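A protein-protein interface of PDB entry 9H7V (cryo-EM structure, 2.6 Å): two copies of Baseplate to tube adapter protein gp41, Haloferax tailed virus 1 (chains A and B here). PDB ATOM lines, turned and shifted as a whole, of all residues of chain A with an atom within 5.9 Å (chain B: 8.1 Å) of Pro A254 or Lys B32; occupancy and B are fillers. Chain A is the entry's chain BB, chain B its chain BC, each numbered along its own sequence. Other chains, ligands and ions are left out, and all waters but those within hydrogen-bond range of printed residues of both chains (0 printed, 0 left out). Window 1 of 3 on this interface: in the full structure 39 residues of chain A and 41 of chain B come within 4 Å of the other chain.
NZ of Lys B32 touches O of Phe A228, at 3.8 Å. Gln A231 touches Asp B50 (CA to OD2, 3.5 Å). Gln A231 touches Ser B51 (CG to C, 3.7 Å). Gln A231 touches Ser B53. CD1 of Leu A232 touches CE of Lys B32, at 3.8 Å. Ser A257 touches Thr B29. Ser A257 touches Gly B31 (O to CA, 3.8 Å). Ser A257 touches Leu B55 (O to CD2, 3.7 Å). CG2 of Thr B29 touches OG of Ser A258 (3.4 Å). Pro A259 touches Gly B31 (CD to CA, 3.7 Å).
The backbone carbonyl oxygen (O) of Val A227 sits close to the side-chain amino group (NZ) of Lys B32 (3.1 Å). NZ of Lys B32 lies within hydrogen-bond range of O of Glu A230 (2.8 Å). The side-chain amide nitrogen (NE2) of Gln A231 lies within hydrogen-bond range of the backbone carbonyl oxygen (O) of Trp B52. The backbone NH (N) of Leu A232 is in hydrogen-bond range of the side-chain carboxylate (OD2) of Asp B50. The backbone NH of Lys B32 is in hydrogen-bond range of the backbone carbonyl oxygen of Gly A256.
N of Ile A253 sits at hydrogen-bond distance from O of Arg A279. N of Glu A277 is in hydrogen-bond range of O of Pro A259 (2.8 Å). O of Gly B31 lies within hydrogen-bond range of N of Leu B55, 2.9 Å away. NZ of Lys B32 is in salt-bridge range of OD2 of Asp B50. N of Gly B54 sits at hydrogen-bond distance from O of Ala B191, at 2.9 Å.
Along chain A the printed residues that touch a printed residue of chain B span positions 227 to 279. Hydrophobic or aromatic side chains of chain B within 4 Å of the printed part of chain A: Phe B30, Val B37, Val B48, Leu B55 and Ala B191. Among the printed residues, 25 pairs touch across the chains.
Pro A254 touches just one residue of chain B: Lys B32. Gly A256 touches three residues of chain B. Printed residues of chain A within 4 Å of Phe B30: Phe A228 (3.8 Å) and Pro A259 (3.3 Å). Of the printed residues of chain B, Gln A231 touches Asp B50 (3.5 Å), Ser B51 (3.7 Å), Trp B52 (2.7 Å) and Ser B53 (3.8 Å). Ala A252 touches none of the printed residues of chain B. Gln B56 touches none of the printed residues of chain A.
No position is printed for both chains. Of the 25 pairs that touch across the chains among the printed residues, none has its exchanged pair printed and touching as well.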
ATOM      1  N   VAL A 227      -5.766 -23.316  10.566  1.00  0.00           N
ATOM      2  CA  VAL A 227      -6.540 -24.106   9.617  1.00  0.00           C
ATOM      3  C   VAL A 227      -7.226 -25.274  10.327  1.00  0.00           C
ATOM      4  O   VAL A 227      -8.420 -25.475  10.130  1.00  0.00           O
ATOM      5  CB  VAL A 227      -5.717 -24.541   8.384  1.00  0.00           C
ATOM      6  CG1 VAL A 227      -6.539 -25.357   7.399  1.00  0.00           C
ATOM      7  CG2 VAL A 227      -5.084 -23.353   7.672  1.00  0.00           C
ATOM      8  N   PHE A 228      -6.492 -26.006  11.178  1.00  0.00           N
ATOM      9  CA  PHE A 228      -6.963 -27.279  11.708  1.00  0.00           C
ATOM     10  C   PHE A 228      -7.585 -27.151  13.097  1.00  0.00           C
ATOM     11  O   PHE A 228      -8.526 -27.879  13.412  1.00  0.00           O
ATOM     12  CB  PHE A 228      -5.871 -28.346  11.620  1.00  0.00           C
ATOM     13  CG  PHE A 228      -5.663 -28.834  10.212  1.00  0.00           C
ATOM     14  CD1 PHE A 228      -6.530 -29.761   9.650  1.00  0.00           C
ATOM     15  CD2 PHE A 228      -4.632 -28.327   9.431  1.00  0.00           C
ATOM     16  CE1 PHE A 228      -6.356 -30.192   8.344  1.00  0.00           C
ATOM     17  CE2 PHE A 228      -4.459 -28.758   8.124  1.00  0.00           C
ATOM     18  CZ  PHE A 228      -5.321 -29.689   7.586  1.00  0.00           C
ATOM     19  N   ARG A 229      -7.061 -26.230  13.914  1.00  0.00           N
ATOM     20  CA  ARG A 229      -7.529 -26.065  15.283  1.00  0.00           C
ATOM     21  C   ARG A 229      -8.531 -24.913  15.376  1.00  0.00           C
ATOM     22  O   ARG A 229      -8.915 -24.512  16.476  1.00  0.00           O
ATOM     23  CB  ARG A 229      -6.346 -25.948  16.251  1.00  0.00           C
ATOM     24  CG  ARG A 229      -5.455 -27.183  16.278  1.00  0.00           C
ATOM     25  CD  ARG A 229      -4.597 -27.321  17.520  1.00  0.00           C
ATOM     26  NE  ARG A 229      -5.329 -27.857  18.661  1.00  0.00           N
ATOM     27  CZ  ARG A 229      -5.507 -27.233  19.823  1.00  0.00           C
ATOM     28  NH1 ARG A 229      -6.189 -27.821  20.789  1.00  0.00           N
ATOM     29  NH2 ARG A 229      -5.001 -26.028  20.022  1.00  0.00           N
ATOM     30  N   GLU A 230      -8.964 -24.404  14.214  1.00  0.00           N
ATOM     31  CA  GLU A 230     -10.006 -23.390  14.125  1.00  0.00           C
ATOM     32  C   GLU A 230     -11.196 -23.929  13.334  1.00  0.00           C
ATOM     33  O   GLU A 230     -11.031 -24.790  12.470  1.00  0.00           O
ATOM     34  CB  GLU A 230      -9.479 -22.118  13.454  1.00  0.00           C
ATOM     35  CG  GLU A 230      -8.726 -21.187  14.392  1.00  0.00           C
ATOM     36  CD  GLU A 230      -9.455 -20.704  15.638  1.00  0.00           C
ATOM     37  OE1 GLU A 230     -10.706 -20.690  15.639  1.00  0.00           O
ATOM     38  OE2 GLU A 230      -8.766 -20.339  16.611  1.00  0.00           O
ATOM     39  N   GLN A 231     -12.389 -23.408  13.647  1.00  0.00           N
ATOM     40  CA  GLN A 231     -13.584 -23.632  12.849  1.00  0.00           C
ATOM     41  C   GLN A 231     -13.621 -22.581  11.744  1.00  0.00           C
ATOM     42  O   GLN A 231     -13.646 -21.383  12.027  1.00  0.00           O
ATOM     43  CB  GLN A 231     -14.845 -23.575  13.716  1.00  0.00           C
ATOM     44  CG  GLN A 231     -15.110 -24.843  14.518  1.00  0.00           C
ATOM     45  CD  GLN A 231     -14.212 -24.996  15.722  1.00  0.00           C
ATOM     46  OE1 GLN A 231     -14.023 -24.070  16.507  1.00  0.00           O
ATOM     47  NE2 GLN A 231     -13.649 -26.182  15.879  1.00  0.00           N
ATOM     48  N   LEU A 232     -13.618 -23.045  10.489  1.00  0.00           N
ATOM     49  CA  LEU A 232     -13.441 -22.172   9.337  1.00  0.00           C
ATOM     50  C   LEU A 232     -14.780 -21.608   8.861  1.00  0.00           C
ATOM     51  O   LEU A 232     -14.802 -20.686   8.045  1.00  0.00           O
ATOM     52  CB  LEU A 232     -12.710 -22.933   8.222  1.00  0.00           C
ATOM     53  CG  LEU A 232     -11.253 -23.310   8.504  1.00  0.00           C
ATOM     54  CD1 LEU A 232     -10.725 -24.255   7.437  1.00  0.00           C
ATOM     55  CD2 LEU A 232     -10.364 -22.078   8.598  1.00  0.00           C
ATOM     56  N   VAL A 237      -9.966 -21.804   3.477  1.00  0.00           N
ATOM     57  CA  VAL A 237      -8.630 -21.325   3.178  1.00  0.00           C
ATOM     58  C   VAL A 237      -8.673 -20.626   1.821  1.00  0.00           C
ATOM     59  O   VAL A 237      -9.369 -21.077   0.913  1.00  0.00           O
ATOM     60  CB  VAL A 237      -7.657 -22.523   3.193  1.00  0.00           C
ATOM     61  CG1 VAL A 237      -6.462 -22.373   2.265  1.00  0.00           C
ATOM     62  CG2 VAL A 237      -7.207 -22.867   4.603  1.00  0.00           C
ATOM     63  N   ALA A 252     -10.572 -23.014  -0.792  1.00  0.00           N
ATOM     64  CA  ALA A 252     -10.461 -24.438  -0.506  1.00  0.00           C
ATOM     65  C   ALA A 252     -10.659 -24.726   0.983  1.00  0.00           C
ATOM     66  O   ALA A 252     -10.731 -23.804   1.791  1.00  0.00           O
ATOM     67  CB  ALA A 252      -9.119 -24.937  -0.988  1.00  0.00           C
ATOM     68  N   ILE A 253     -10.752 -26.021   1.325  1.00  0.00           N
ATOM     69  CA  ILE A 253     -10.796 -26.503   2.701  1.00  0.00           C
ATOM     70  C   ILE A 253     -10.151 -27.892   2.763  1.00  0.00           C
ATOM     71  O   ILE A 253     -10.288 -28.672   1.821  1.00  0.00           O
ATOM     72  CB  ILE A 253     -12.238 -26.480   3.267  1.00  0.00           C
ATOM     73  CG1 ILE A 253     -12.267 -26.515   4.800  1.00  0.00           C
ATOM     74  CG2 ILE A 253     -13.117 -27.566   2.653  1.00  0.00           C
ATOM     75  CD1 ILE A 253     -13.525 -25.945   5.419  1.00  0.00           C
ATOM     76  N   PRO A 254      -9.390 -28.237   3.833  1.00  0.00           N
ATOM     77  CA  PRO A 254      -8.993 -29.627   4.075  1.00  0.00           C
ATOM     78  C   PRO A 254     -10.178 -30.495   4.499  1.00  0.00           C
ATOM     79  O   PRO A 254     -10.909 -30.137   5.421  1.00  0.00           O
ATOM     80  CB  PRO A 254      -7.979 -29.525   5.223  1.00  0.00           C
ATOM     81  CG  PRO A 254      -7.543 -28.079   5.212  1.00  0.00           C
ATOM     82  CD  PRO A 254      -8.778 -27.311   4.800  1.00  0.00           C
ATOM     83  N   VAL A 255     -10.350 -31.637   3.819  1.00  0.00           N
ATOM     84  CA  VAL A 255     -11.526 -32.482   3.978  1.00  0.00           C
ATOM     85  C   VAL A 255     -11.110 -33.830   4.563  1.00  0.00           C
ATOM     86  O   VAL A 255     -10.138 -34.433   4.111  1.00  0.00           O
ATOM     87  CB  VAL A 255     -12.289 -32.656   2.645  1.00  0.00           C
ATOM     88  CG1 VAL A 255     -13.513 -33.551   2.782  1.00  0.00           C
ATOM     89  CG2 VAL A 255     -12.684 -31.322   2.031  1.00  0.00           C
ATOM     90  N   GLY A 256     -11.864 -34.287   5.572  1.00  0.00           N
ATOM     91  CA  GLY A 256     -11.815 -35.670   6.018  1.00  0.00           C
ATOM     92  C   GLY A 256     -10.830 -35.905   7.159  1.00  0.00           C
ATOM     93  O   GLY A 256     -10.469 -34.976   7.880  1.00  0.00           O
ATOM     94  N   SER A 257     -10.397 -37.166   7.287  1.00  0.00           N
ATOM     95  CA  SER A 257      -9.704 -37.662   8.465  1.00  0.00           C
ATOM     96  C   SER A 257      -8.186 -37.531   8.343  1.00  0.00           C
ATOM     97  O   SER A 257      -7.495 -37.536   9.361  1.00  0.00           O
ATOM     98  CB  SER A 257     -10.113 -39.083   8.772  1.00  0.00           C
ATOM     99  OG  SER A 257      -9.874 -39.932   7.659  1.00  0.00           O
ATOM    100  N   SER A 258      -7.670 -37.404   7.109  1.00  0.00           N
ATOM    101  CA  SER A 258      -6.230 -37.456   6.889  1.00  0.00           C
ATOM    102  C   SER A 258      -5.733 -36.462   5.831  1.00  0.00           C
ATOM    103  O   SER A 258      -4.835 -36.809   5.061  1.00  0.00           O
ATOM    104  CB  SER A 258      -5.810 -38.871   6.570  1.00  0.00           C
ATOM    105  OG  SER A 258      -4.399 -39.002   6.629  1.00  0.00           O
ATOM    106  N   PRO A 259      -6.237 -35.202   5.753  1.00  0.00           N
ATOM    107  CA  PRO A 259      -5.749 -34.245   4.755  1.00  0.00           C
ATOM    108  C   PRO A 259      -4.352 -33.661   4.981  1.00  0.00           C
ATOM    109  O   PRO A 259      -3.731 -33.203   4.025  1.00  0.00           O
ATOM    110  CB  PRO A 259      -6.807 -33.133   4.768  1.00  0.00           C
ATOM    111  CG  PRO A 259      -7.359 -33.167   6.172  1.00  0.00           C
ATOM    112  CD  PRO A 259      -7.319 -34.628   6.570  1.00  0.00           C
ATOM    113  N   LEU A 276      -0.637 -32.576   2.000  1.00  0.00           N
ATOM    114  CA  LEU A 276      -1.515 -31.492   2.404  1.00  0.00           C
ATOM    115  C   LEU A 276      -2.565 -31.327   1.308  1.00  0.00           C
ATOM    116  O   LEU A 276      -2.256 -30.871   0.208  1.00  0.00           O
ATOM    117  CB  LEU A 276      -0.695 -30.216   2.639  1.00  0.00           C
ATOM    118  CG  LEU A 276      -1.481 -28.935   2.927  1.00  0.00           C
ATOM    119  CD1 LEU A 276      -2.348 -29.059   4.173  1.00  0.00           C
ATOM    120  CD2 LEU A 276      -0.543 -27.745   3.056  1.00  0.00           C
ATOM    121  N   GLU A 277      -3.803 -31.726   1.628  1.00  0.00           N
ATOM    122  CA  GLU A 277      -4.845 -31.946   0.638  1.00  0.00           C
ATOM    123  C   GLU A 277      -5.977 -30.939   0.836  1.00  0.00           C
ATOM    124  O   GLU A 277      -6.532 -30.824   1.928  1.00  0.00           O
ATOM    125  CB  GLU A 277      -5.331 -33.396   0.731  1.00  0.00           C
ATOM    126  CG  GLU A 277      -6.285 -33.802  -0.375  1.00  0.00           C
ATOM    127  CD  GLU A 277      -6.799 -35.231  -0.297  1.00  0.00           C
ATOM    128  OE1 GLU A 277      -6.033 -36.119   0.136  1.00  0.00           O
ATOM    129  OE2 GLU A 277      -7.967 -35.456  -0.674  1.00  0.00           O
ATOM    130  N   PHE A 278      -6.309 -30.231  -0.251  1.00  0.00           N
ATOM    131  CA  PHE A 278      -7.301 -29.167  -0.258  1.00  0.00           C
ATOM    132  C   PHE A 278      -8.353 -29.446  -1.327  1.00  0.00           C
ATOM    133  O   PHE A 278      -8.007 -29.652  -2.489  1.00  0.00           O
ATOM    134  CB  PHE A 278      -6.631 -27.829  -0.580  1.00  0.00           C
ATOM    135  CG  PHE A 278      -5.822 -27.221   0.537  1.00  0.00           C
ATOM    136  CD1 PHE A 278      -6.451 -26.703   1.661  1.00  0.00           C
ATOM    137  CD2 PHE A 278      -4.438 -27.145   0.460  1.00  0.00           C
ATOM    138  CE1 PHE A 278      -5.714 -26.137   2.692  1.00  0.00           C
ATOM    139  CE2 PHE A 278      -3.702 -26.573   1.489  1.00  0.00           C
ATOM    140  CZ  PHE A 278      -4.340 -26.073   2.604  1.00  0.00           C
ATOM    141  N   ARG A 279      -9.633 -29.442  -0.929  1.00  0.00           N
ATOM    142  CA  ARG A 279     -10.721 -29.460  -1.898  1.00  0.00           C
ATOM    143  C   ARG A 279     -11.213 -28.036  -2.138  1.00  0.00           C
ATOM    144  O   ARG A 279     -11.433 -27.287  -1.190  1.00  0.00           O
ATOM    145  CB  ARG A 279     -11.881 -30.364  -1.471  1.00  0.00           C
ATOM    146  CG  ARG A 279     -12.947 -30.510  -2.549  1.00  0.00           C
ATOM    147  CD  ARG A 279     -14.004 -31.563  -2.304  1.00  0.00           C
ATOM    148  NE  ARG A 279     -14.972 -31.548  -3.392  1.00  0.00           N
ATOM    149  CZ  ARG A 279     -15.984 -32.399  -3.530  1.00  0.00           C
ATOM    150  NH1 ARG A 279     -16.801 -32.285  -4.562  1.00  0.00           N
ATOM    151  NH2 ARG A 279     -16.179 -33.360  -2.644  1.00  0.00           N
ATOM    152  N   THR B  29      -1.273 -36.823  12.320  1.00  0.00           N
ATOM    153  CA  THR B  29      -2.293 -36.583  11.313  1.00  0.00           C
ATOM    154  C   THR B  29      -3.310 -35.586  11.862  1.00  0.00           C
ATOM    155  O   THR B  29      -3.866 -35.791  12.939  1.00  0.00           O
ATOM    156  CB  THR B  29      -2.970 -37.892  10.879  1.00  0.00           C
ATOM    157  OG1 THR B  29      -1.970 -38.816  10.449  1.00  0.00           O
ATOM    158  CG2 THR B  29      -3.989 -37.707   9.777  1.00  0.00           C
ATOM    159  N   PHE B  30      -3.533 -34.509  11.100  1.00  0.00           N
ATOM    160  CA  PHE B  30      -4.569 -33.534  11.391  1.00  0.00           C
ATOM    161  C   PHE B  30      -5.717 -33.735  10.412  1.00  0.00           C
ATOM    162  O   PHE B  30      -5.490 -33.936   9.220  1.00  0.00           O
ATOM    163  CB  PHE B  30      -4.032 -32.107  11.270  1.00  0.00           C
ATOM    164  CG  PHE B  30      -2.962 -31.747  12.267  1.00  0.00           C
ATOM    165  CD1 PHE B  30      -1.663 -32.210  12.110  1.00  0.00           C
ATOM    166  CD2 PHE B  30      -3.249 -30.936  13.358  1.00  0.00           C
ATOM    167  CE1 PHE B  30      -0.675 -31.885  13.028  1.00  0.00           C
ATOM    168  CE2 PHE B  30      -2.259 -30.606  14.272  1.00  0.00           C
ATOM    169  CZ  PHE B  30      -0.975 -31.078  14.104  1.00  0.00           C
ATOM    170  N   GLY B  31      -6.943 -33.672  10.936  1.00  0.00           N
ATOM    171  CA  GLY B  31      -8.126 -33.871  10.122  1.00  0.00           C
ATOM    172  C   GLY B  31      -9.299 -33.015  10.582  1.00  0.00           C
ATOM    173  O   GLY B  31      -9.275 -32.431  11.665  1.00  0.00           O
ATOM    174  N   LYS B  32     -10.313 -32.956   9.716  1.00  0.00           N
ATOM    175  CA  LYS B  32     -11.609 -32.382  10.025  1.00  0.00           C
ATOM    176  C   LYS B  32     -12.673 -33.409   9.647  1.00  0.00           C
ATOM    177  O   LYS B  32     -13.317 -33.267   8.609  1.00  0.00           O
ATOM    178  CB  LYS B  32     -11.799 -31.075   9.251  1.00  0.00           C
ATOM    179  CG  LYS B  32     -10.880 -29.931   9.650  1.00  0.00           C
ATOM    180  CD  LYS B  32     -11.140 -28.679   8.851  1.00  0.00           C
ATOM    181  CE  LYS B  32     -10.456 -27.460   9.429  1.00  0.00           C
ATOM    182  NZ  LYS B  32     -11.063 -27.028  10.710  1.00  0.00           N
ATOM    183  N   PRO B  33     -12.882 -34.490  10.443  1.00  0.00           N
ATOM    184  CA  PRO B  33     -13.870 -35.517  10.103  1.00  0.00           C
ATOM    185  C   PRO B  33     -15.294 -34.970  10.018  1.00  0.00           C
ATOM    186  O   PRO B  33     -16.166 -35.607   9.428  1.00  0.00           O
ATOM    187  CB  PRO B  33     -13.787 -36.510  11.272  1.00  0.00           C
ATOM    188  CG  PRO B  33     -12.414 -36.282  11.857  1.00  0.00           C
ATOM    189  CD  PRO B  33     -12.186 -34.794  11.704  1.00  0.00           C
ATOM    190  N   GLU B  34     -15.496 -33.773  10.584  1.00  0.00           N
ATOM    191  CA  GLU B  34     -16.819 -33.229  10.842  1.00  0.00           C
ATOM    192  C   GLU B  34     -17.162 -32.083   9.890  1.00  0.00           C
ATOM    193  O   GLU B  34     -18.185 -31.426  10.081  1.00  0.00           O
ATOM    194  CB  GLU B  34     -16.938 -32.785  12.304  1.00  0.00           C
ATOM    195  CG  GLU B  34     -16.819 -33.915  13.318  1.00  0.00           C
ATOM    196  CD  GLU B  34     -17.753 -35.103  13.143  1.00  0.00           C
ATOM    197  OE1 GLU B  34     -18.938 -34.894  12.805  1.00  0.00           O
ATOM    198  OE2 GLU B  34     -17.289 -36.243  13.342  1.00  0.00           O
ATOM    199  N   VAL B  35     -16.324 -31.840   8.870  1.00  0.00           N
ATOM    200  CA  VAL B  35     -16.713 -30.899   7.830  1.00  0.00           C
ATOM    201  C   VAL B  35     -17.821 -31.528   6.993  1.00  0.00           C
ATOM    202  O   VAL B  35     -17.742 -32.696   6.614  1.00  0.00           O
ATOM    203  CB  VAL B  35     -15.556 -30.383   6.948  1.00  0.00           C
ATOM    204  CG1 VAL B  35     -14.701 -29.348   7.660  1.00  0.00           C
ATOM    205  CG2 VAL B  35     -14.699 -31.489   6.346  1.00  0.00           C
ATOM    206  N   ASN B  36     -18.863 -30.731   6.747  1.00  0.00           N
ATOM    207  CA  ASN B  36     -19.890 -31.097   5.791  1.00  0.00           C
ATOM    208  C   ASN B  36     -19.534 -30.470   4.449  1.00  0.00           C
ATOM    209  O   ASN B  36     -19.577 -29.250   4.300  1.00  0.00           O
ATOM    210  CB  ASN B  36     -21.290 -30.729   6.286  1.00  0.00           C
ATOM    211  CG  ASN B  36     -21.732 -31.556   7.474  1.00  0.00           C
ATOM    212  OD1 ASN B  36     -21.905 -32.769   7.365  1.00  0.00           O
ATOM    213  ND2 ASN B  36     -21.926 -30.911   8.612  1.00  0.00           N
ATOM    214  N   VAL B  37     -19.141 -31.331   3.507  1.00  0.00           N
ATOM    215  CA  VAL B  37     -18.961 -30.965   2.112  1.00  0.00           C
ATOM    216  C   VAL B  37     -20.184 -31.482   1.361  1.00  0.00           C
ATOM    217  O   VAL B  37     -20.537 -32.654   1.484  1.00  0.00           O
ATOM    218  CB  VAL B  37     -17.648 -31.538   1.539  1.00  0.00           C
ATOM    219  CG1 VAL B  37     -17.433 -31.152   0.083  1.00  0.00           C
ATOM    220  CG2 VAL B  37     -16.439 -31.141   2.370  1.00  0.00           C
ATOM    221  N   VAL B  48     -19.525 -25.674   1.839  1.00  0.00           N
ATOM    222  CA  VAL B  48     -19.029 -26.407   2.993  1.00  0.00           C
ATOM    223  C   VAL B  48     -19.488 -25.712   4.274  1.00  0.00           C
ATOM    224  O   VAL B  48     -19.866 -24.541   4.250  1.00  0.00           O
ATOM    225  CB  VAL B  48     -17.494 -26.575   2.971  1.00  0.00           C
ATOM    226  CG1 VAL B  48     -17.020 -27.463   1.832  1.00  0.00           C
ATOM    227  CG2 VAL B  48     -16.748 -25.247   2.976  1.00  0.00           C
ATOM    228  N   ILE B  49     -19.445 -26.461   5.382  1.00  0.00           N
ATOM    229  CA  ILE B  49     -19.566 -25.900   6.719  1.00  0.00           C
ATOM    230  C   ILE B  49     -18.652 -26.669   7.674  1.00  0.00           C
ATOM    231  O   ILE B  49     -18.621 -27.899   7.670  1.00  0.00           O
ATOM    232  CB  ILE B  49     -21.036 -25.797   7.196  1.00  0.00           C
ATOM    233  CG1 ILE B  49     -21.173 -25.308   8.643  1.00  0.00           C
ATOM    234  CG2 ILE B  49     -21.808 -27.088   6.956  1.00  0.00           C
ATOM    235  CD1 ILE B  49     -21.002 -23.815   8.823  1.00  0.00           C
ATOM    236  N   ASP B  50     -17.908 -25.897   8.473  1.00  0.00           N
ATOM    237  CA  ASP B  50     -16.971 -26.381   9.472  1.00  0.00           C
ATOM    238  C   ASP B  50     -17.384 -25.797  10.822  1.00  0.00           C
ATOM    239  O   ASP B  50     -17.305 -24.585  11.020  1.00  0.00           O
ATOM    240  CB  ASP B  50     -15.542 -26.005   9.066  1.00  0.00           C
ATOM    241  CG  ASP B  50     -14.453 -26.455  10.028  1.00  0.00           C
ATOM    242  OD1 ASP B  50     -14.653 -27.475  10.722  1.00  0.00           O
ATOM    243  OD2 ASP B  50     -13.406 -25.783  10.068  1.00  0.00           O
ATOM    244  N   SER B  51     -17.822 -26.667  11.745  1.00  0.00           N
ATOM    245  CA  SER B  51     -18.573 -26.219  12.910  1.00  0.00           C
ATOM    246  C   SER B  51     -18.142 -26.922  14.199  1.00  0.00           C
ATOM    247  O   SER B  51     -18.611 -26.558  15.278  1.00  0.00           O
ATOM    248  CB  SER B  51     -20.056 -26.373  12.666  1.00  0.00           C
ATOM    249  OG  SER B  51     -20.806 -25.702  13.667  1.00  0.00           O
ATOM    250  N   TRP B  52     -17.240 -27.904  14.086  1.00  0.00           N
ATOM    251  CA  TRP B  52     -16.946 -28.822  15.175  1.00  0.00           C
ATOM    252  C   TRP B  52     -15.435 -28.931  15.395  1.00  0.00           C
ATOM    253  O   TRP B  52     -14.652 -28.356  14.640  1.00  0.00           O
ATOM    254  CB  TRP B  52     -17.558 -30.196  14.874  1.00  0.00           C
ATOM    255  CG  TRP B  52     -19.039 -30.247  14.639  1.00  0.00           C
ATOM    256  CD1 TRP B  52     -19.691 -30.153  13.443  1.00  0.00           C
ATOM    257  CD2 TRP B  52     -20.057 -30.486  15.626  1.00  0.00           C
ATOM    258  NE1 TRP B  52     -21.043 -30.290  13.622  1.00  0.00           N
ATOM    259  CE2 TRP B  52     -21.298 -30.497  14.951  1.00  0.00           C
ATOM    260  CE3 TRP B  52     -20.044 -30.676  17.014  1.00  0.00           C
ATOM    261  CZ2 TRP B  52     -22.507 -30.695  15.621  1.00  0.00           C
ATOM    262  CZ3 TRP B  52     -21.238 -30.874  17.675  1.00  0.00           C
ATOM    263  CH2 TRP B  52     -22.452 -30.883  16.986  1.00  0.00           C
ATOM    264  N   SER B  53     -15.051 -29.690  16.434  1.00  0.00           N
ATOM    265  CA  SER B  53     -13.669 -29.993  16.776  1.00  0.00           C
ATOM    266  C   SER B  53     -12.977 -30.725  15.629  1.00  0.00           C
ATOM    267  O   SER B  53     -13.619 -31.458  14.879  1.00  0.00           O
ATOM    268  CB  SER B  53     -13.601 -30.797  18.050  1.00  0.00           C
ATOM    269  OG  SER B  53     -14.422 -31.953  17.965  1.00  0.00           O
ATOM    270  N   GLY B  54     -11.661 -30.515  15.511  1.00  0.00           N
ATOM    271  CA  GLY B  54     -10.847 -31.245  14.554  1.00  0.00           C
ATOM    272  C   GLY B  54     -10.466 -32.625  15.083  1.00  0.00           C
ATOM    273  O   GLY B  54     -11.032 -33.102  16.064  1.00  0.00           O
ATOM    274  N   LEU B  55      -9.501 -33.250  14.402  1.00  0.00           N
ATOM    275  CA  LEU B  55      -8.867 -34.481  14.843  1.00  0.00           C
ATOM    276  C   LEU B  55      -7.355 -34.282  14.791  1.00  0.00           C
ATOM    277  O   LEU B  55      -6.836 -33.760  13.807  1.00  0.00           O
ATOM    278  CB  LEU B  55      -9.310 -35.620  13.914  1.00  0.00           C
ATOM    279  CG  LEU B  55      -8.582 -36.959  14.060  1.00  0.00           C
ATOM    280  CD1 LEU B  55      -9.069 -37.730  15.277  1.00  0.00           C
ATOM    281  CD2 LEU B  55      -8.749 -37.802  12.805  1.00  0.00           C
ATOM    282  N   GLN B  56      -6.668 -34.679  15.867  1.00  0.00           N
ATOM    283  CA  GLN B  56      -5.224 -34.845  15.835  1.00  0.00           C
ATOM    284  C   GLN B  56      -4.879 -36.235  16.361  1.00  0.00           C
ATOM    285  O   GLN B  56      -5.274 -36.601  17.466  1.00  0.00           O
ATOM    286  CB  GLN B  56      -4.496 -33.731  16.591  1.00  0.00           C
ATOM    287  CG  GLN B  56      -2.980 -33.801  16.441  1.00  0.00           C
ATOM    288  CD  GLN B  56      -2.228 -32.621  17.009  1.00  0.00           C
ATOM    289  OE1 GLN B  56      -2.808 -31.660  17.508  1.00  0.00           O
ATOM    290  NE2 GLN B  56      -0.910 -32.676  16.913  1.00  0.00           N
ATOM    291  N   ALA B 191     -11.335 -26.710  19.720  1.00  0.00           N
ATOM    292  CA  ALA B 191     -10.378 -27.371  18.843  1.00  0.00           C
ATOM    293  C   ALA B 191     -10.418 -28.894  18.977  1.00  0.00           C
ATOM    294  O   ALA B 191     -10.346 -29.593  17.968  1.00  0.00           O
ATOM    295  CB  ALA B 191      -8.991 -26.822  19.077  1.00  0.00           C
